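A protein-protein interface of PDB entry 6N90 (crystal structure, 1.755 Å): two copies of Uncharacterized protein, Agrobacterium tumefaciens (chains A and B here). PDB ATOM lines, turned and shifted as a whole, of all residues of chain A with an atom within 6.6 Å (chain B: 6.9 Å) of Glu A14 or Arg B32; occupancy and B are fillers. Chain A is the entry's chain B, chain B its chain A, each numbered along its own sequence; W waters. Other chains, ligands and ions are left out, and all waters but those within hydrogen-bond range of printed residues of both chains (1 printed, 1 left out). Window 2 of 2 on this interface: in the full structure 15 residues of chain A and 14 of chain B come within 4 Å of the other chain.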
ATOM      1  N   SER A   9     -31.820 -16.125  13.349  1.00  0.00           N
ATOM      2  CA  SER A   9     -31.934 -15.366  12.084  1.00  0.00           C
ATOM      3  C   SER A   9     -31.125 -15.986  10.941  1.00  0.00           C
ATOM      4  O   SER A   9     -31.535 -15.900   9.767  1.00  0.00           O
ATOM      5  CB  SER A   9     -31.525 -13.910  12.288  1.00  0.00           C
ATOM      6  OG  SER A   9     -30.128 -13.783  12.482  1.00  0.00           O
ATOM      7  N   TRP A  10     -30.009 -16.642  11.246  1.00  0.00           N
ATOM      8  CA  TRP A  10     -29.302 -17.376  10.188  1.00  0.00           C
ATOM      9  C   TRP A  10     -30.159 -18.559   9.738  1.00  0.00           C
ATOM     10  O   TRP A  10     -30.189 -18.898   8.545  1.00  0.00           O
ATOM     11  CB  TRP A  10     -27.907 -17.851  10.644  1.00  0.00           C
ATOM     12  CG  TRP A  10     -27.134 -18.475   9.520  1.00  0.00           C
ATOM     13  CD1 TRP A  10     -26.760 -19.789   9.402  1.00  0.00           C
ATOM     14  CD2 TRP A  10     -26.645 -17.812   8.350  1.00  0.00           C
ATOM     15  NE1 TRP A  10     -26.063 -19.977   8.229  1.00  0.00           N
ATOM     16  CE2 TRP A  10     -25.989 -18.784   7.559  1.00  0.00           C
ATOM     17  CE3 TRP A  10     -26.721 -16.489   7.878  1.00  0.00           C
ATOM     18  CZ2 TRP A  10     -25.402 -18.479   6.323  1.00  0.00           C
ATOM     19  CZ3 TRP A  10     -26.117 -16.185   6.645  1.00  0.00           C
ATOM     20  CH2 TRP A  10     -25.477 -17.183   5.887  1.00  0.00           C
ATOM     21  N   ASP A  11     -30.878 -19.178  10.671  1.00  0.00           N
ATOM     22  CA  ASP A  11     -31.730 -20.303  10.282  1.00  0.00           C
ATOM     23  C   ASP A  11     -32.851 -19.805   9.347  1.00  0.00           C
ATOM     24  O   ASP A  11     -33.208 -20.484   8.336  1.00  0.00           O
ATOM     25  CB  ASP A  11     -32.312 -21.017  11.514  1.00  0.00           C
ATOM     26  CG  ASP A  11     -33.090 -22.245  11.127  1.00  0.00           C
ATOM     27  OD1 ASP A  11     -32.453 -23.298  10.968  1.00  0.00           O
ATOM     28  OD2 ASP A  11     -34.324 -22.138  10.916  1.00  0.00           O
ATOM     29  N   ASP A  12     -33.376 -18.622   9.663  1.00  0.00           N
ATOM     30  CA  ASP A  12     -34.380 -17.941   8.816  1.00  0.00           C
ATOM     31  C   ASP A  12     -33.831 -17.750   7.394  1.00  0.00           C
ATOM     32  O   ASP A  12     -34.486 -18.051   6.374  1.00  0.00           O
ATOM     33  CB  ASP A  12     -34.739 -16.544   9.371  1.00  0.00           C
ATOM     34  CG  ASP A  12     -35.602 -16.564  10.645  1.00  0.00           C
ATOM     35  OD1 ASP A  12     -36.208 -17.606  10.976  1.00  0.00           O
ATOM     36  OD2 ASP A  12     -35.713 -15.482  11.279  1.00  0.00           O
ATOM     37  N   TYR A  13     -32.611 -17.227   7.344  1.00  0.00           N
ATOM     38  CA  TYR A  13     -31.999 -16.889   6.064  1.00  0.00           C
ATOM     39  C   TYR A  13     -31.761 -18.148   5.240  1.00  0.00           C
ATOM     40  O   TYR A  13     -32.020 -18.165   4.034  1.00  0.00           O
ATOM     41  CB  TYR A  13     -30.693 -16.158   6.295  1.00  0.00           C
ATOM     42  CG  TYR A  13     -30.053 -15.573   5.064  1.00  0.00           C
ATOM     43  CD1 TYR A  13     -30.594 -14.451   4.430  1.00  0.00           C
ATOM     44  CD2 TYR A  13     -28.861 -16.095   4.586  1.00  0.00           C
ATOM     45  CE1 TYR A  13     -29.960 -13.877   3.332  1.00  0.00           C
ATOM     46  CE2 TYR A  13     -28.234 -15.554   3.475  1.00  0.00           C
ATOM     47  CZ  TYR A  13     -28.793 -14.450   2.848  1.00  0.00           C
ATOM     48  OH  TYR A  13     -28.127 -13.893   1.777  1.00  0.00           O
ATOM     49  N   GLU A  14     -31.240 -19.191   5.888  1.00  0.00           N
ATOM     50  CA  GLU A  14     -31.042 -20.490   5.234  1.00  0.00           C
ATOM     51  C   GLU A  14     -32.347 -21.077   4.734  1.00  0.00           C
ATOM     52  O   GLU A  14     -32.372 -21.727   3.705  1.00  0.00           O
ATOM     53  CB  GLU A  14     -30.412 -21.496   6.195  1.00  0.00           C
ATOM     54  CG  GLU A  14     -28.953 -21.281   6.444  1.00  0.00           C
ATOM     55  CD  GLU A  14     -28.352 -22.501   7.092  1.00  0.00           C
ATOM     56  OE1 GLU A  14     -27.440 -23.089   6.486  1.00  0.00           O
ATOM     57  OE2 GLU A  14     -28.810 -22.878   8.200  1.00  0.00           O
ATOM     58  N   PHE A  15     -33.411 -20.870   5.505  1.00  0.00           N
ATOM     59  CA  PHE A  15     -34.734 -21.364   5.148  1.00  0.00           C
ATOM     60  C   PHE A  15     -35.151 -20.690   3.841  1.00  0.00           C
ATOM     61  O   PHE A  15     -35.665 -21.353   2.952  1.00  0.00           O
ATOM     62  CB  PHE A  15     -35.753 -21.090   6.254  1.00  0.00           C
ATOM     63  CG  PHE A  15     -37.185 -21.306   5.809  1.00  0.00           C
ATOM     64  CD1 PHE A  15     -37.718 -22.589   5.737  1.00  0.00           C
ATOM     65  CD2 PHE A  15     -37.964 -20.230   5.422  1.00  0.00           C
ATOM     66  CE1 PHE A  15     -39.027 -22.784   5.302  1.00  0.00           C
ATOM     67  CE2 PHE A  15     -39.271 -20.416   4.988  1.00  0.00           C
ATOM     68  CZ  PHE A  15     -39.795 -21.703   4.922  1.00  0.00           C
ATOM     69  N   TRP A  16     -34.918 -19.385   3.737  1.00  0.00           N
ATOM     70  CA  TRP A  16     -35.257 -18.676   2.497  1.00  0.00           C
ATOM     71  C   TRP A  16     -34.357 -19.148   1.355  1.00  0.00           C
ATOM     72  O   TRP A  16     -34.806 -19.239   0.197  1.00  0.00           O
ATOM     73  CB  TRP A  16     -35.155 -17.162   2.675  1.00  0.00           C
ATOM     74  CG  TRP A  16     -36.219 -16.597   3.589  1.00  0.00           C
ATOM     75  CD1 TRP A  16     -36.030 -15.811   4.704  1.00  0.00           C
ATOM     76  CD2 TRP A  16     -37.638 -16.787   3.471  1.00  0.00           C
ATOM     77  NE1 TRP A  16     -37.256 -15.481   5.263  1.00  0.00           N
ATOM     78  CE2 TRP A  16     -38.251 -16.079   4.530  1.00  0.00           C
ATOM     79  CE3 TRP A  16     -38.446 -17.501   2.584  1.00  0.00           C
ATOM     80  CZ2 TRP A  16     -39.633 -16.061   4.710  1.00  0.00           C
ATOM     81  CZ3 TRP A  16     -39.830 -17.462   2.761  1.00  0.00           C
ATOM     82  CH2 TRP A  16     -40.399 -16.747   3.817  1.00  0.00           C
ATOM     83  N   GLN A  17     -33.088 -19.422   1.654  1.00  0.00           N
ATOM     84  CA  GLN A  17     -32.195 -19.888   0.596  1.00  0.00           C
ATOM     85  C   GLN A  17     -32.714 -21.219   0.031  1.00  0.00           C
ATOM     86  O   GLN A  17     -32.561 -21.507  -1.162  1.00  0.00           O
ATOM     87  CB  GLN A  17     -30.763 -20.029   1.107  1.00  0.00           C
ATOM     88  CG  GLN A  17     -30.066 -18.709   1.404  1.00  0.00           C
ATOM     89  CD  GLN A  17     -28.619 -18.927   1.870  1.00  0.00           C
ATOM     90  OE1 GLN A  17     -28.358 -19.738   2.760  1.00  0.00           O
ATOM     91  NE2 GLN A  17     -27.685 -18.201   1.272  1.00  0.00           N
ATOM     92  N   ARG A  18     -33.346 -22.011   0.894  1.00  0.00           N
ATOM     93  CA  ARG A  18     -33.798 -23.353   0.540  1.00  0.00           C
ATOM     94  C   ARG A  18     -35.146 -23.307  -0.186  1.00  0.00           C
ATOM     95  O   ARG A  18     -35.474 -24.231  -0.927  1.00  0.00           O
ATOM     96  CB  ARG A  18     -33.922 -24.223   1.798  1.00  0.00           C
ATOM     97  CG  ARG A  18     -33.092 -25.511   1.783  1.00  0.00           C
ATOM     98  CD  ARG A  18     -33.046 -26.185   3.153  1.00  0.00           C
ATOM     99  NE  ARG A  18     -34.374 -26.329   3.745  1.00  0.00           N
ATOM    100  CZ  ARG A  18     -34.742 -25.778   4.899  1.00  0.00           C
ATOM    101  NH1 ARG A  18     -33.879 -25.059   5.607  1.00  0.00           N
ATOM    102  NH2 ARG A  18     -35.974 -25.957   5.354  1.00  0.00           N
ATOM    103  N   THR A  19     -35.916 -22.240   0.021  1.00  0.00           N
ATOM    104  CA  THR A  19     -37.341 -22.253  -0.358  1.00  0.00           C
ATOM    105  C   THR A  19     -37.831 -21.092  -1.231  1.00  0.00           C
ATOM    106  O   THR A  19     -38.857 -21.229  -1.915  1.00  0.00           O
ATOM    107  CB  THR A  19     -38.258 -22.267   0.898  1.00  0.00           C
ATOM    108  OG1 THR A  19     -38.130 -21.029   1.606  1.00  0.00           O
ATOM    109  CG2 THR A  19     -37.917 -23.386   1.814  1.00  0.00           C
ATOM    110  N   VAL A  24     -34.620 -14.113  -0.375  1.00  0.00           N
ATOM    111  CA  VAL A  24     -33.169 -13.954  -0.160  1.00  0.00           C
ATOM    112  C   VAL A  24     -32.710 -12.640  -0.805  1.00  0.00           C
ATOM    113  O   VAL A  24     -31.992 -11.852  -0.197  1.00  0.00           O
ATOM    114  CB  VAL A  24     -32.358 -15.135  -0.757  1.00  0.00           C
ATOM    115  CG1 VAL A  24     -30.845 -14.885  -0.587  1.00  0.00           C
ATOM    116  CG2 VAL A  24     -32.743 -16.443  -0.079  1.00  0.00           C
ATOM    117  N   CYS A  84     -35.616 -12.617  10.326  1.00  0.00           N
ATOM    118  CA  CYS A  84     -36.056 -12.252   8.972  1.00  0.00           C
ATOM    119  C   CYS A  84     -37.092 -13.227   8.423  1.00  0.00           C
ATOM    120  O   CYS A  84     -37.148 -13.491   7.220  1.00  0.00           O
ATOM    121  CB  CYS A  84     -34.867 -12.136   8.008  1.00  0.00           C
ATOM    122  SG  CYS A  84     -33.838 -13.599   7.739  1.00  0.00           S
ATOM    123  N   TYR B  13     -19.521 -13.775  -0.425  1.00  0.00           N
ATOM    124  CA  TYR B  13     -20.654 -14.704  -0.284  1.00  0.00           C
ATOM    125  C   TYR B  13     -21.773 -14.301  -1.232  1.00  0.00           C
ATOM    126  O   TYR B  13     -22.369 -15.154  -1.872  1.00  0.00           O
ATOM    127  CB  TYR B  13     -21.158 -14.708   1.150  1.00  0.00           C
ATOM    128  CG  TYR B  13     -22.237 -15.721   1.511  1.00  0.00           C
ATOM    129  CD1 TYR B  13     -21.953 -17.084   1.615  1.00  0.00           C
ATOM    130  CD2 TYR B  13     -23.508 -15.282   1.863  1.00  0.00           C
ATOM    131  CE1 TYR B  13     -22.946 -17.996   2.013  1.00  0.00           C
ATOM    132  CE2 TYR B  13     -24.503 -16.172   2.246  1.00  0.00           C
ATOM    133  CZ  TYR B  13     -24.227 -17.523   2.308  1.00  0.00           C
ATOM    134  OH  TYR B  13     -25.227 -18.390   2.707  1.00  0.00           O
ATOM    135  N   GLU B  25     -23.883 -23.332  -1.065  1.00  0.00           N
ATOM    136  CA  GLU B  25     -24.258 -24.507  -0.286  1.00  0.00           C
ATOM    137  C   GLU B  25     -23.076 -25.123   0.450  1.00  0.00           C
ATOM    138  O   GLU B  25     -23.209 -25.557   1.596  1.00  0.00           O
ATOM    139  CB  GLU B  25     -24.900 -25.559  -1.193  1.00  0.00           C
ATOM    140  CG  GLU B  25     -26.203 -25.108  -1.817  1.00  0.00           C
ATOM    141  N   ILE B  27     -20.382 -23.520   1.421  1.00  0.00           N
ATOM    142  CA  ILE B  27     -20.034 -22.601   2.497  1.00  0.00           C
ATOM    143  C   ILE B  27     -21.034 -22.741   3.677  1.00  0.00           C
ATOM    144  O   ILE B  27     -20.657 -22.779   4.832  1.00  0.00           O
ATOM    145  CB  ILE B  27     -19.989 -21.151   1.961  1.00  0.00           C
ATOM    146  CG1 ILE B  27     -18.789 -20.937   1.027  1.00  0.00           C
ATOM    147  CG2 ILE B  27     -19.990 -20.126   3.083  1.00  0.00           C
ATOM    148  CD1 ILE B  27     -18.933 -19.629   0.107  1.00  0.00           C
ATOM    149  N   ASN B  28     -22.326 -22.850   3.385  1.00  0.00           N
ATOM    150  CA  ASN B  28     -23.284 -23.058   4.461  1.00  0.00           C
ATOM    151  C   ASN B  28     -23.015 -24.334   5.244  1.00  0.00           C
ATOM    152  O   ASN B  28     -23.236 -24.366   6.455  1.00  0.00           O
ATOM    153  CB  ASN B  28     -24.712 -23.076   3.886  1.00  0.00           C
ATOM    154  CG  ASN B  28     -25.163 -21.699   3.446  1.00  0.00           C
ATOM    155  OD1 ASN B  28     -24.425 -20.727   3.570  1.00  0.00           O
ATOM    156  ND2 ASN B  28     -26.368 -21.611   2.889  1.00  0.00           N
ATOM    157  N   ASP B  29     -22.543 -25.377   4.559  1.00  0.00           N
ATOM    158  CA  ASP B  29     -22.204 -26.659   5.195  1.00  0.00           C
ATOM    159  C   ASP B  29     -20.964 -26.478   6.070  1.00  0.00           C
ATOM    160  O   ASP B  29     -20.861 -27.031   7.162  1.00  0.00           O
ATOM    161  CB  ASP B  29     -21.975 -27.745   4.115  1.00  0.00           C
ATOM    162  CG  ASP B  29     -22.441 -29.143   4.551  1.00  0.00           C
ATOM    163  OD1 ASP B  29     -22.919 -29.296   5.695  1.00  0.00           O
ATOM    164  OD2 ASP B  29     -22.304 -30.109   3.762  1.00  0.00           O
ATOM    165  N   LEU B  30     -20.013 -25.689   5.586  1.00  0.00           N
ATOM    166  CA  LEU B  30     -18.799 -25.458   6.348  1.00  0.00           C
ATOM    167  C   LEU B  30     -19.145 -24.681   7.620  1.00  0.00           C
ATOM    168  O   LEU B  30     -18.640 -24.965   8.711  1.00  0.00           O
ATOM    169  CB  LEU B  30     -17.777 -24.707   5.473  1.00  0.00           C
ATOM    170  CG  LEU B  30     -17.107 -25.535   4.363  1.00  0.00           C
ATOM    171  CD1 LEU B  30     -16.237 -24.660   3.451  1.00  0.00           C
ATOM    172  CD2 LEU B  30     -16.296 -26.690   4.918  1.00  0.00           C
ATOM    173  N   ILE B  31     -20.035 -23.701   7.475  1.00  0.00           N
ATOM    174  CA  ILE B  31     -20.503 -22.915   8.621  1.00  0.00           C
ATOM    175  C   ILE B  31     -21.181 -23.805   9.678  1.00  0.00           C
ATOM    176  O   ILE B  31     -20.795 -23.791  10.882  1.00  0.00           O
ATOM    177  CB  ILE B  31     -21.472 -21.801   8.154  1.00  0.00           C
ATOM    178  CG1 ILE B  31     -20.714 -20.751   7.346  1.00  0.00           C
ATOM    179  CG2 ILE B  31     -22.214 -21.145   9.352  1.00  0.00           C
ATOM    180  CD1 ILE B  31     -21.566 -19.688   6.735  1.00  0.00           C
ATOM    181  N   ARG B  32     -22.174 -24.574   9.228  1.00  0.00           N
ATOM    182  CA  ARG B  32     -22.899 -25.510  10.084  1.00  0.00           C
ATOM    183  C   ARG B  32     -21.901 -26.401  10.839  1.00  0.00           C
ATOM    184  O   ARG B  32     -22.004 -26.582  12.054  1.00  0.00           O
ATOM    185  CB  ARG B  32     -23.866 -26.361   9.244  1.00  0.00           C
ATOM    186  CG  ARG B  32     -24.967 -27.091  10.025  1.00  0.00           C
ATOM    187  CD  ARG B  32     -25.951 -27.767   9.017  1.00  0.00           C
ATOM    188  NE  ARG B  32     -26.361 -26.816   7.975  1.00  0.00           N
ATOM    189  CZ  ARG B  32     -26.215 -26.994   6.660  1.00  0.00           C
ATOM    190  NH1 ARG B  32     -25.690 -28.116   6.177  1.00  0.00           N
ATOM    191  NH2 ARG B  32     -26.629 -26.065   5.801  1.00  0.00           N
ATOM    192  N   ASN B  33     -20.901 -26.910  10.120  1.00  0.00           N
ATOM    193  CA  ASN B  33     -19.959 -27.864  10.706  1.00  0.00           C
ATOM    194  C   ASN B  33     -19.012 -27.185  11.696  1.00  0.00           C
ATOM    195  O   ASN B  33     -18.760 -27.711  12.789  1.00  0.00           O
ATOM    196  CB  ASN B  33     -19.160 -28.573   9.607  1.00  0.00           C
ATOM    197  CG  ASN B  33     -19.854 -29.830   9.074  1.00  0.00           C
ATOM    198  OD1 ASN B  33     -19.520 -30.947   9.473  1.00  0.00           O
ATOM    199  ND2 ASN B  33     -20.814 -29.652   8.159  1.00  0.00           N
ATOM    200  N   ALA B  34     -18.515 -26.005  11.330  1.00  0.00           N
ATOM    201  CA  ALA B  34     -17.559 -25.286  12.177  1.00  0.00           C
ATOM    202  C   ALA B  34     -18.214 -24.761  13.456  1.00  0.00           C
ATOM    203  O   ALA B  34     -17.548 -24.592  14.482  1.00  0.00           O
ATOM    204  CB  ALA B  34     -16.917 -24.141  11.397  1.00  0.00           C
ATOM    205  N   LYS B  35     -19.513 -24.467  13.389  1.00  0.00           N
ATOM    206  CA  LYS B  35     -20.233 -24.044  14.585  1.00  0.00           C
ATOM    207  C   LYS B  35     -20.345 -25.223  15.554  1.00  0.00           C
ATOM    208  O   LYS B  35     -20.245 -25.031  16.765  1.00  0.00           O
ATOM    209  CB  LYS B  35     -21.611 -23.482  14.231  1.00  0.00           C
ATOM    210  CG  LYS B  35     -21.557 -22.037  13.789  1.00  0.00           C
ATOM    211  CD  LYS B  35     -22.786 -21.633  12.949  1.00  0.00           C
ATOM    212  CE  LYS B  35     -24.066 -22.133  13.546  1.00  0.00           C
ATOM    213  NZ  LYS B  35     -25.242 -21.931  12.602  1.00  0.00           N
ATOM    214  N   ARG B  36     -20.502 -26.436  15.020  1.00  0.00           N
ATOM    215  CA  ARG B  36     -20.581 -27.653  15.841  1.00  0.00           C
ATOM    216  C   ARG B  36     -19.210 -28.111  16.364  1.00  0.00           C
ATOM    217  O   ARG B  36     -19.005 -28.272  17.571  1.00  0.00           O
ATOM    218  CB  ARG B  36     -21.222 -28.798  15.048  1.00  0.00           C
ATOM    219  CG  ARG B  36     -22.727 -28.721  14.927  1.00  0.00           C
ATOM    220  CD  ARG B  36     -23.267 -29.915  14.147  1.00  0.00           C
ATOM    221  NE  ARG B  36     -22.752 -29.934  12.778  1.00  0.00           N
ATOM    222  CZ  ARG B  36     -23.502 -30.077  11.687  1.00  0.00           C
ATOM    223  NH1 ARG B  36     -24.818 -30.218  11.791  1.00  0.00           N
ATOM    224  NH2 ARG B  36     -22.931 -30.076  10.489  1.00  0.00           N
ATOM    225  N   THR B  37     -18.294 -28.344  15.431  1.00  0.00           N
ATOM    226  CA  THR B  37     -16.956 -28.822  15.729  1.00  0.00           C
ATOM    227  C   THR B  37     -15.927 -27.905  15.067  1.00  0.00           C
ATOM    228  O   THR B  37     -15.467 -28.196  13.982  1.00  0.00           O
ATOM    229  CB  THR B  37     -16.759 -30.272  15.227  1.00  0.00           C
ATOM    230  OG1 THR B  37     -17.089 -30.355  13.829  1.00  0.00           O
ATOM    231  CG2 THR B  37     -17.669 -31.223  15.984  1.00  0.00           C
ATOM    232  N   PHE B  66     -12.226 -21.236   3.027  1.00  0.00           N
ATOM    233  CA  PHE B  66     -13.128 -20.669   4.023  1.00  0.00           C
ATOM    234  C   PHE B  66     -12.265 -20.440   5.249  1.00  0.00           C
ATOM    235  O   PHE B  66     -11.831 -21.400   5.881  1.00  0.00           O
ATOM    236  CB  PHE B  66     -14.308 -21.649   4.279  1.00  0.00           C
ATOM    237  CG  PHE B  66     -15.243 -21.262   5.418  1.00  0.00           C
ATOM    238  CD1 PHE B  66     -16.270 -20.362   5.222  1.00  0.00           C
ATOM    239  CD2 PHE B  66     -15.121 -21.865   6.669  1.00  0.00           C
ATOM    240  CE1 PHE B  66     -17.146 -20.035   6.246  1.00  0.00           C
ATOM    241  CE2 PHE B  66     -15.982 -21.523   7.717  1.00  0.00           C
ATOM    242  CZ  PHE B  66     -16.997 -20.607   7.497  1.00  0.00           C
ATOM    243  N   LEU B  79     -18.753 -17.272  15.454  1.00  0.00           N
ATOM    244  CA  LEU B  79     -17.884 -17.698  14.376  1.00  0.00           C
ATOM    245  C   LEU B  79     -17.721 -16.499  13.475  1.00  0.00           C
ATOM    246  O   LEU B  79     -18.710 -15.959  12.995  1.00  0.00           O
ATOM    247  CB  LEU B  79     -18.477 -18.872  13.585  1.00  0.00           C
ATOM    248  CG  LEU B  79     -17.518 -19.486  12.559  1.00  0.00           C
ATOM    249  CD1 LEU B  79     -17.798 -20.964  12.392  1.00  0.00           C
ATOM    250  CD2 LEU B  79     -17.659 -18.796  11.224  1.00  0.00           C
HETATM  251  O   HOH W   1     -25.204 -22.775   7.706  1.00  0.00           O
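Water W1 lies within hydrogen-bond range of the side-chain carboxylate (OE1) of Glu A14, the backbone carbonyl oxygen (O) of Asn B28 and the indole nitrogen (NE1) of Trp A10.
Of the printed residues of chain B, Trp A10 touches Tyr B13 and Asn B28.
Printed residues of chain B within 4 Å of Tyr A13: Tyr B13 (3.98 Å).
Of the printed residues of chain B, Glu A14 touches Asn B28 and Arg B32.
Printed residues of chain B within 4 Å of Gln A17: Tyr B13 (2.9 Å) and Asn B28 (2.7 Å).
Of the printed residues of chain A, Tyr B13 touches Trp A10 (3.4 Å), Tyr A13 (3.98 Å) and Gln A17 (2.9 Å).
Of the printed residues of chain A, Asn B28 touches Trp A10 (3.7 Å), Glu A14 (3.8 Å) and Gln A17 (2.7 Å).
Of the printed residues of chain A, Arg B32 touches Glu A14.
The nearest residue of chain A that does not touch Arg B32 is Trp A10 (6.1 Å).
The side-chain hydroxyl (OH) of Tyr B13 is in hydrogen-bond range of the side-chain amide nitrogen (NE2) of Gln A17, at 2.9 Å.
ND2 of Asn B28 lies within hydrogen-bond range of OE1 of Gln A17, at 2.7 Å.
The guanidinium group (NH2) of Arg B32 is in salt-bridge range of the side-chain carboxylate (OE1) of Glu A14 (3.2 Å).
The side-chain hydroxyl of Tyr B13 sits at hydrogen-bond distance from the side-chain amide oxygen of Asn B28, 2.6 Å away.
OD1 of Asp B29 lies within salt-bridge range of NH1 of Arg B32, 3.1 Å away.
Tyr A13 touches its own counterpart, Tyr B13.
Of the 15 printed residues of chain B, 3 touch a printed residue of chain A.
Hydrophobic or aromatic side chains of chain A that line the printed part of chain B: Trp A10 and Tyr A13.
Among the printed residues, 7 pairs touch across the chains.
Among the printed residues, Asp or Glu carboxylates within 4 Å of a Lys or Arg side-chain nitrogen of the other chain: Glu A14 with Arg B32 (3.2 Å).
Tyr B13 touches Trp A10.
Trp A10 touches Asn B28 (CZ2 to OD1, 3.7 Å).
CE2 of Tyr B13 touches CE2 of Tyr A13 (3.98 Å).
Asn B28 touches Glu A14.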
